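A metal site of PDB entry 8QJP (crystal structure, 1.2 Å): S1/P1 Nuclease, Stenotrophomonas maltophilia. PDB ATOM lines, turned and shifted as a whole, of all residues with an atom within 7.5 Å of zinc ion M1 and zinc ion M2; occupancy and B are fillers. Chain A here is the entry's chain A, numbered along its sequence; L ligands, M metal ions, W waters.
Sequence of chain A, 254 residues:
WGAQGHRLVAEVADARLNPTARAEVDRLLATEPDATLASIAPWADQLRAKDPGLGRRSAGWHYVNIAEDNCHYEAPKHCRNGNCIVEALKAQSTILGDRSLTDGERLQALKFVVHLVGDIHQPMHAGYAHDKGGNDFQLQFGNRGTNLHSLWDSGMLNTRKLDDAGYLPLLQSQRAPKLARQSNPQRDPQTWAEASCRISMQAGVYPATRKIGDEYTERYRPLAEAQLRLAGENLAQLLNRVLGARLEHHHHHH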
ATOM      1  N   TRP A   1       1.865 -13.644  26.972  1.00  0.00           N
ATOM      2  CA  TRP A   1       2.750 -12.814  27.795  1.00  0.00           C
ATOM      3  C   TRP A   1       3.886 -12.317  26.936  1.00  0.00           C
ATOM      4  O   TRP A   1       4.202 -12.929  25.891  1.00  0.00           O
ATOM      5  CB  TRP A   1       3.351 -13.607  28.986  1.00  0.00           C
ATOM      6  CG  TRP A   1       2.340 -14.261  29.868  1.00  0.00           C
ATOM      7  CD1 TRP A   1       1.904 -15.548  29.808  1.00  0.00           C
ATOM      8  CD2 TRP A   1       1.617 -13.648  30.942  1.00  0.00           C
ATOM      9  NE1 TRP A   1       0.997 -15.804  30.796  1.00  0.00           N
ATOM     10  CE2 TRP A   1       0.784 -14.649  31.511  1.00  0.00           C
ATOM     11  CE3 TRP A   1       1.617 -12.369  31.509  1.00  0.00           C
ATOM     12  CZ2 TRP A   1      -0.045 -14.407  32.589  1.00  0.00           C
ATOM     13  CZ3 TRP A   1       0.821 -12.133  32.586  1.00  0.00           C
ATOM     14  CH2 TRP A   1      -0.019 -13.130  33.094  1.00  0.00           C
ATOM     15  N   GLY A   2       4.554 -11.277  27.420  1.00  0.00           N
ATOM     16  CA  GLY A   2       5.896 -10.918  26.941  1.00  0.00           C
ATOM     17  C   GLY A   2       6.937 -11.865  27.487  1.00  0.00           C
ATOM     18  O   GLY A   2       6.606 -12.840  28.200  1.00  0.00           O
ATOM     19  N   ALA A   3       8.198 -11.600  27.198  1.00  0.00           N
ATOM     20  CA  ALA A   3       9.276 -12.564  27.448  1.00  0.00           C
ATOM     21  C   ALA A   3       9.401 -12.835  28.957  1.00  0.00           C
ATOM     22  O   ALA A   3       9.558 -14.000  29.343  1.00  0.00           O
ATOM     23  CB  ALA A   3      10.572 -12.074  26.835  1.00  0.00           C
ATOM     24  N   GLY A   5       7.159 -12.658  31.409  1.00  0.00           N
ATOM     25  CA  GLY A   5       6.079 -13.539  31.913  1.00  0.00           C
ATOM     26  C   GLY A   5       6.349 -14.987  31.513  1.00  0.00           C
ATOM     27  O   GLY A   5       6.167 -15.892  32.325  1.00  0.00           O
ATOM     28  N   HIS A   6       6.771 -15.224  30.276  1.00  0.00           N
ATOM     29  CA  HIS A   6       7.055 -16.600  29.830  1.00  0.00           C
ATOM     30  C   HIS A   6       8.186 -17.242  30.650  1.00  0.00           C
ATOM     31  O   HIS A   6       8.065 -18.389  31.078  1.00  0.00           O
ATOM     32  CB  HIS A   6       7.363 -16.663  28.334  1.00  0.00           C
ATOM     33  CG  HIS A   6       6.102 -16.548  27.551  1.00  0.00           C
ATOM     34  ND1 HIS A   6       5.178 -17.574  27.534  1.00  0.00           N
ATOM     35  CD2 HIS A   6       5.573 -15.546  26.819  1.00  0.00           C
ATOM     36  CE1 HIS A   6       4.132 -17.179  26.803  1.00  0.00           C
ATOM     37  NE2 HIS A   6       4.327 -15.918  26.378  1.00  0.00           N
ATOM     38  N   ALA A  41      11.613 -20.352  27.058  1.00  0.00           N
ATOM     39  CA  ALA A  41      10.178 -20.058  27.246  1.00  0.00           C
ATOM     40  C   ALA A  41       9.669 -19.018  26.249  1.00  0.00           C
ATOM     41  O   ALA A  41       8.535 -19.149  25.808  1.00  0.00           O
ATOM     42  CB  ALA A  41       9.873 -19.674  28.668  1.00  0.00           C
ATOM     43  N   PRO A  42      10.425 -17.959  25.885  1.00  0.00           N
ATOM     44  CA  PRO A  42       9.965 -16.993  24.903  1.00  0.00           C
ATOM     45  C   PRO A  42      10.127 -17.397  23.439  1.00  0.00           C
ATOM     46  O   PRO A  42       9.667 -16.686  22.556  1.00  0.00           O
ATOM     47  CB  PRO A  42      10.870 -15.759  25.165  1.00  0.00           C
ATOM     48  CG  PRO A  42      11.436 -15.971  26.546  1.00  0.00           C
ATOM     49  CD  PRO A  42      11.627 -17.462  26.618  1.00  0.00           C
ATOM     50  N   ALA A  44       8.878 -19.354  21.195  1.00  0.00           N
ATOM     51  CA  ALA A  44       7.805 -19.460  20.201  1.00  0.00           C
ATOM     52  C   ALA A  44       7.403 -18.078  19.698  1.00  0.00           C
ATOM     53  O   ALA A  44       6.821 -18.006  18.624  1.00  0.00           O
ATOM     54  CB  ALA A  44       6.639 -20.216  20.768  1.00  0.00           C
ATOM     55  N   ASP A  45       7.599 -17.009  20.490  1.00  0.00           N
ATOM     56  CA  ASP A  45       7.287 -15.613  20.034  1.00  0.00           C
ATOM     57  C   ASP A  45       8.365 -15.042  19.114  1.00  0.00           C
ATOM     58  O   ASP A  45       8.105 -13.976  18.499  1.00  0.00           O
ATOM     59  CB  ASP A  45       7.067 -14.696  21.227  1.00  0.00           C
ATOM     60  CG  ASP A  45       5.727 -14.803  21.917  1.00  0.00           C
ATOM     61  OD1 ASP A  45       4.829 -15.475  21.400  1.00  0.00           O
ATOM     62  OD2 ASP A  45       5.564 -14.235  23.033  1.00  0.00           O
ATOM     63  N   GLN A  46       9.521 -15.680  19.027  1.00  0.00           N
ATOM     64  CA  GLN A  46      10.711 -15.136  18.326  1.00  0.00           C
ATOM     65  C   GLN A  46      10.844 -15.722  16.913  1.00  0.00           C
ATOM     66  O   GLN A  46      11.826 -15.401  16.262  1.00  0.00           O
ATOM     67  CB  GLN A  46      11.942 -15.392  19.199  1.00  0.00           C
ATOM     68  CG  GLN A  46      11.862 -14.736  20.575  1.00  0.00           C
ATOM     69  CD  GLN A  46      12.939 -15.155  21.538  1.00  0.00           C
ATOM     70  OE1 GLN A  46      13.447 -16.281  21.491  1.00  0.00           O
ATOM     71  NE2 GLN A  46      13.303 -14.250  22.445  1.00  0.00           N
ATOM     72  N   ALA A  59       1.566 -19.132  14.354  1.00  0.00           N
ATOM     73  CA  ALA A  59       1.169 -17.808  14.896  1.00  0.00           C
ATOM     74  C   ALA A  59      -0.168 -17.892  15.659  1.00  0.00           C
ATOM     75  O   ALA A  59      -0.308 -17.298  16.775  1.00  0.00           O
ATOM     76  CB  ALA A  59       1.113 -16.781  13.803  1.00  0.00           C
ATOM     77  N   TRP A  61      -1.422 -20.341  17.178  1.00  0.00           N
ATOM     78  CA  TRP A  61      -1.380 -21.300  18.304  1.00  0.00           C
ATOM     79  C   TRP A  61      -1.297 -20.568  19.642  1.00  0.00           C
ATOM     80  O   TRP A  61      -1.407 -21.238  20.652  1.00  0.00           O
ATOM     81  CB  TRP A  61      -0.196 -22.244  18.168  1.00  0.00           C
ATOM     82  CG  TRP A  61      -0.209 -23.122  16.971  1.00  0.00           C
ATOM     83  CD1 TRP A  61      -1.094 -23.134  15.920  1.00  0.00           C
ATOM     84  CD2 TRP A  61       0.796 -24.094  16.693  1.00  0.00           C
ATOM     85  NE1 TRP A  61      -0.723 -24.110  15.030  1.00  0.00           N
ATOM     86  CE2 TRP A  61       0.443 -24.706  15.473  1.00  0.00           C
ATOM     87  CE3 TRP A  61       1.954 -24.522  17.360  1.00  0.00           C
ATOM     88  CZ2 TRP A  61       1.220 -25.713  14.906  1.00  0.00           C
ATOM     89  CZ3 TRP A  61       2.719 -25.511  16.788  1.00  0.00           C
ATOM     90  CH2 TRP A  61       2.341 -26.108  15.586  1.00  0.00           C
ATOM     91  N   HIS A  62      -1.052 -19.259  19.624  1.00  0.00           N
ATOM     92  CA  HIS A  62      -0.811 -18.530  20.898  1.00  0.00           C
ATOM     93  C   HIS A  62      -2.104 -18.119  21.585  1.00  0.00           C
ATOM     94  O   HIS A  62      -2.006 -17.599  22.720  1.00  0.00           O
ATOM     95  CB  HIS A  62       0.095 -17.338  20.674  1.00  0.00           C
ATOM     96  CG  HIS A  62       1.459 -17.706  20.226  1.00  0.00           C
ATOM     97  ND1 HIS A  62       2.600 -17.318  20.911  1.00  0.00           N
ATOM     98  CD2 HIS A  62       1.863 -18.366  19.114  1.00  0.00           C
ATOM     99  CE1 HIS A  62       3.654 -17.815  20.266  1.00  0.00           C
ATOM    100  NE2 HIS A  62       3.218 -18.458  19.155  1.00  0.00           N
ATOM    101  N   TYR A  63      -3.255 -18.265  20.949  1.00  0.00           N
ATOM    102  CA  TYR A  63      -4.492 -17.728  21.553  1.00  0.00           C
ATOM    103  C   TYR A  63      -5.723 -18.495  21.092  1.00  0.00           C
ATOM    104  O   TYR A  63      -5.644 -19.363  20.228  1.00  0.00           O
ATOM    105  CB  TYR A  63      -4.610 -16.246  21.263  1.00  0.00           C
ATOM    106  CG  TYR A  63      -4.610 -15.953  19.804  1.00  0.00           C
ATOM    107  CD1 TYR A  63      -3.427 -15.798  19.105  1.00  0.00           C
ATOM    108  CD2 TYR A  63      -5.806 -15.810  19.110  1.00  0.00           C
ATOM    109  CE1 TYR A  63      -3.462 -15.557  17.741  1.00  0.00           C
ATOM    110  CE2 TYR A  63      -5.854 -15.541  17.763  1.00  0.00           C
ATOM    111  CZ  TYR A  63      -4.672 -15.409  17.064  1.00  0.00           C
ATOM    112  OH  TYR A  63      -4.774 -15.146  15.721  1.00  0.00           O
ATOM    113  N   ILE A  85      -4.748 -22.189  20.526  1.00  0.00           N
ATOM    114  CA  ILE A  85      -3.894 -22.668  21.633  1.00  0.00           C
ATOM    115  C   ILE A  85      -4.411 -23.952  22.245  1.00  0.00           C
ATOM    116  O   ILE A  85      -3.611 -24.722  22.754  1.00  0.00           O
ATOM    117  CB  ILE A  85      -3.704 -21.557  22.666  1.00  0.00           C
ATOM    118  CG1 ILE A  85      -2.563 -21.915  23.640  1.00  0.00           C
ATOM    119  CG2 ILE A  85      -4.988 -21.201  23.402  1.00  0.00           C
ATOM    120  CD1 ILE A  85      -1.964 -20.723  24.312  1.00  0.00           C
ATOM    121  N   HIS A 115       5.877 -22.547  26.379  1.00  0.00           N
ATOM    122  CA  HIS A 115       5.343 -21.230  25.977  1.00  0.00           C
ATOM    123  C   HIS A 115       3.816 -21.228  26.120  1.00  0.00           C
ATOM    124  O   HIS A 115       3.225 -20.266  26.618  1.00  0.00           O
ATOM    125  CB  HIS A 115       5.754 -20.925  24.542  1.00  0.00           C
ATOM    126  CG  HIS A 115       5.409 -19.545  24.136  1.00  0.00           C
ATOM    127  ND1 HIS A 115       6.270 -18.498  24.346  1.00  0.00           N
ATOM    128  CD2 HIS A 115       4.304 -19.007  23.569  1.00  0.00           C
ATOM    129  CE1 HIS A 115       5.707 -17.380  23.904  1.00  0.00           C
ATOM    130  NE2 HIS A 115       4.477 -17.660  23.417  1.00  0.00           N
ATOM    131  N   LEU A 116       3.200 -22.271  25.536  1.00  0.00           N
ATOM    132  CA  LEU A 116       1.736 -22.278  25.416  1.00  0.00           C
ATOM    133  C   LEU A 116       1.064 -22.449  26.775  1.00  0.00           C
ATOM    134  O   LEU A 116      -0.028 -21.890  26.959  1.00  0.00           O
ATOM    135  CB  LEU A 116       1.273 -23.291  24.381  1.00  0.00           C
ATOM    136  CG  LEU A 116       1.722 -23.028  22.937  1.00  0.00           C
ATOM    137  CD1 LEU A 116       1.200 -24.118  22.021  1.00  0.00           C
ATOM    138  CD2 LEU A 116       1.323 -21.664  22.417  1.00  0.00           C
ATOM    139  N   GLY A 118       2.095 -21.004  29.340  1.00  0.00           N
ATOM    140  CA  GLY A 118       2.071 -19.591  29.747  1.00  0.00           C
ATOM    141  C   GLY A 118       0.918 -18.849  29.058  1.00  0.00           C
ATOM    142  O   GLY A 118       0.125 -18.190  29.722  1.00  0.00           O
ATOM    143  N   ASP A 119       0.884 -18.872  27.724  1.00  0.00           N
ATOM    144  CA  ASP A 119      -0.087 -18.055  26.965  1.00  0.00           C
ATOM    145  C   ASP A 119      -1.528 -18.436  27.308  1.00  0.00           C
ATOM    146  O   ASP A 119      -2.397 -17.553  27.343  1.00  0.00           O
ATOM    147  CB  ASP A 119       0.127 -18.158  25.463  1.00  0.00           C
ATOM    148  CG  ASP A 119       1.099 -17.150  24.907  1.00  0.00           C
ATOM    149  OD1 ASP A 119       1.497 -16.216  25.695  1.00  0.00           O
ATOM    150  OD2 ASP A 119       1.537 -17.307  23.718  1.00  0.00           O
ATOM    151  N   ILE A 120      -1.811 -19.698  27.592  1.00  0.00           N
ATOM    152  CA  ILE A 120      -3.207 -20.122  27.823  1.00  0.00           C
ATOM    153  C   ILE A 120      -3.697 -19.658  29.196  1.00  0.00           C
ATOM    154  O   ILE A 120      -4.888 -19.738  29.450  1.00  0.00           O
ATOM    155  CB  ILE A 120      -3.342 -21.652  27.608  1.00  0.00           C
ATOM    156  CG1 ILE A 120      -4.785 -22.055  27.268  1.00  0.00           C
ATOM    157  CG2 ILE A 120      -2.856 -22.426  28.834  1.00  0.00           C
ATOM    158  CD1 ILE A 120      -4.906 -23.480  26.741  1.00  0.00           C
ATOM    159  N   GLN A 122      -2.819 -16.404  30.075  1.00  0.00           N
ATOM    160  CA  GLN A 122      -2.899 -14.946  29.891  1.00  0.00           C
ATOM    161  C   GLN A 122      -4.317 -14.590  29.479  1.00  0.00           C
ATOM    162  O   GLN A 122      -4.748 -14.995  28.399  1.00  0.00           O
ATOM    163  CB  GLN A 122      -1.860 -14.553  28.863  1.00  0.00           C
ATOM    164  CG  GLN A 122      -2.073 -13.162  28.311  1.00  0.00           C
ATOM    165  CD  GLN A 122      -2.249 -12.110  29.372  1.00  0.00           C
ATOM    166  OE1 GLN A 122      -3.286 -11.456  29.453  1.00  0.00           O
ATOM    167  NE2 GLN A 122      -1.233 -11.980  30.220  1.00  0.00           N
ATOM    168  N   HIS A 125      -5.070 -13.582  25.930  1.00  0.00           N
ATOM    169  CA  HIS A 125      -4.874 -14.644  24.913  1.00  0.00           C
ATOM    170  C   HIS A 125      -6.106 -15.557  24.816  1.00  0.00           C
ATOM    171  O   HIS A 125      -6.052 -16.539  24.051  1.00  0.00           O
ATOM    172  CB  HIS A 125      -3.585 -15.416  25.191  1.00  0.00           C
ATOM    173  CG  HIS A 125      -2.356 -14.676  24.738  1.00  0.00           C
ATOM    174  ND1 HIS A 125      -1.449 -15.194  23.830  1.00  0.00           N
ATOM    175  CD2 HIS A 125      -1.878 -13.421  25.053  1.00  0.00           C
ATOM    176  CE1 HIS A 125      -0.496 -14.309  23.574  1.00  0.00           C
ATOM    177  NE2 HIS A 125      -0.721 -13.189  24.313  1.00  0.00           N
ATOM    178  N   HIS A 149      -4.124  -5.471  25.571  1.00  0.00           N
ATOM    179  CA  HIS A 149      -3.378  -6.721  25.385  1.00  0.00           C
ATOM    180  C   HIS A 149      -1.963  -6.598  25.975  1.00  0.00           C
ATOM    181  O   HIS A 149      -1.562  -7.405  26.791  1.00  0.00           O
ATOM    182  CB  HIS A 149      -3.361  -7.150  23.920  1.00  0.00           C
ATOM    183  CG  HIS A 149      -2.792  -8.512  23.746  1.00  0.00           C
ATOM    184  ND1 HIS A 149      -3.580  -9.617  23.580  1.00  0.00           N
ATOM    185  CD2 HIS A 149      -1.504  -8.941  23.729  1.00  0.00           C
ATOM    186  CE1 HIS A 149      -2.812 -10.675  23.490  1.00  0.00           C
ATOM    187  NE2 HIS A 149      -1.517 -10.316  23.567  1.00  0.00           N
ATOM    188  N   ASP A 153       0.044  -8.474  28.942  1.00  0.00           N
ATOM    189  CA  ASP A 153       1.234  -9.281  28.593  1.00  0.00           C
ATOM    190  C   ASP A 153       2.453  -8.829  29.366  1.00  0.00           C
ATOM    191  O   ASP A 153       3.277  -9.686  29.724  1.00  0.00           O
ATOM    192  CB  ASP A 153       1.554  -9.223  27.088  1.00  0.00           C
ATOM    193  CG  ASP A 153       0.900 -10.293  26.215  1.00  0.00           C
ATOM    194  OD1 ASP A 153       0.167 -11.128  26.745  1.00  0.00           O
ATOM    195  OD2 ASP A 153       1.129 -10.247  25.010  1.00  0.00           O
HETATM  196  N1  LIG L   1      -2.205 -12.400  19.127  1.00  0.00           N
HETATM  197  C1  LIG L   1      -3.013 -12.674  20.211  1.00  0.00           C
HETATM  198  N2  LIG L   1      -4.366 -12.535  19.982  1.00  0.00           N
HETATM  199  C2  LIG L   1      -4.973 -12.171  18.801  1.00  0.00           C
HETATM  200  C3  LIG L   1      -4.065 -11.839  17.735  1.00  0.00           C
HETATM  201  C4  LIG L   1      -2.729 -11.965  17.928  1.00  0.00           C
HETATM  202  O1  LIG L   1      -2.590 -13.092  21.290  1.00  0.00           O
HETATM  203  O2  LIG L   1      -6.198 -12.158  18.737  1.00  0.00           O
HETATM  204  C5  LIG L   1      -0.712 -12.583  19.284  1.00  0.00           C
HETATM  205  C6  LIG L   1      -0.290 -14.036  19.183  1.00  0.00           C
HETATM  206  O3  LIG L   1       0.794 -14.245  20.092  1.00  0.00           O
HETATM  207  C7  LIG L   1       0.157 -14.146  17.728  1.00  0.00           C
HETATM  208  C8  LIG L   1       0.802 -12.790  17.497  1.00  0.00           C
HETATM  209  O4  LIG L   1       1.114 -15.160  17.471  1.00  0.00           O
HETATM  210  O5  LIG L   1      -0.018 -11.887  18.266  1.00  0.00           O
HETATM  211  C9  LIG L   1       0.913 -12.332  16.068  1.00  0.00           C
HETATM  212  O6  LIG L   1      -0.384 -12.376  15.438  1.00  0.00           O
HETATM  213  P1  LIG L   1      -0.579 -11.689  14.039  1.00  0.00           P
HETATM  214  O7  LIG L   1      -1.857 -12.253  13.480  1.00  0.00           O
HETATM  215  O8  LIG L   1       0.615 -12.068  13.162  1.00  0.00           O
HETATM  216  O9  LIG L   1      -0.486 -10.183  14.239  1.00  0.00           O
HETATM  217 ZN    ZN M   1       3.058 -16.378  22.645  1.00  0.00          ZN
HETATM  218 ZN    ZN M   2       2.919 -14.727  25.500  1.00  0.00          ZN
HETATM  219 ZN    ZN M   3       0.111 -11.431  23.872  1.00  0.00          ZN
HETATM  220  O   HOH W   1       2.920 -14.679  23.577  1.00  0.00           O
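The backbone carbonyl oxygen (O) of His 62 sits at hydrogen-bond distance from a ring nitrogen (ND1) of His 125 (2.7 Å).
A ring nitrogen (ND1) of His 6 lies close to the backbone carbonyl oxygen (O) of His 115.
A ring nitrogen (ND1) of His 115 lies within hydrogen-bond range of the backbone carbonyl oxygen (O) of Ala 41 (2.8 Å).
OD1 of Asp 153 lies close to N of Trp 1 (3.0 Å).
The indole nitrogen of Trp 1 is in hydrogen-bond range of the backbone carbonyl oxygen of Gly 118, 2.8 Å away.
Water W1 binds zinc ion M1, at 1.9 Å.
ND1 of His 62 binds zinc ion M1 (2.0 Å).
NE2 of His 115 binds zinc ion M1, 2.1 Å away.
OD2 of Asp 119 is bound to zinc ion M1 (2.1 Å).
The side-chain carboxylate (OD1) of Asp 45 binds zinc ion M1 (2.3 Å).
His 125 touches zinc ion M2 (CE1 to ZN, 3.9 Å).
The nearest printed residue that does not touch zinc ion M2 is Gly 2 (4.3 Å).
Within 4 Å of zinc ion M1: His 6, Asp 45, His 62, His 115 and Asp 119.
Along chain A the residues within 4 Å of zinc ion M1 span positions 6 to 119.
O1 of the ligand lies close to ND1 of His 125.
An oxygen (O4) of the ligand is in hydrogen-bond range of the backbone carbonyl oxygen (O) of Ala 59, at 2.7 Å.
Zinc ion M2 is bound by water W1 (1.9 Å), a ring nitrogen (NE2) of His 6 (2.0 Å), the side-chain carboxylate of Asp 119 (2.1 Å), the backbone nitrogen of Trp 1 (2.1 Å) and the backbone carbonyl oxygen of Trp 1 (2.2 Å).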
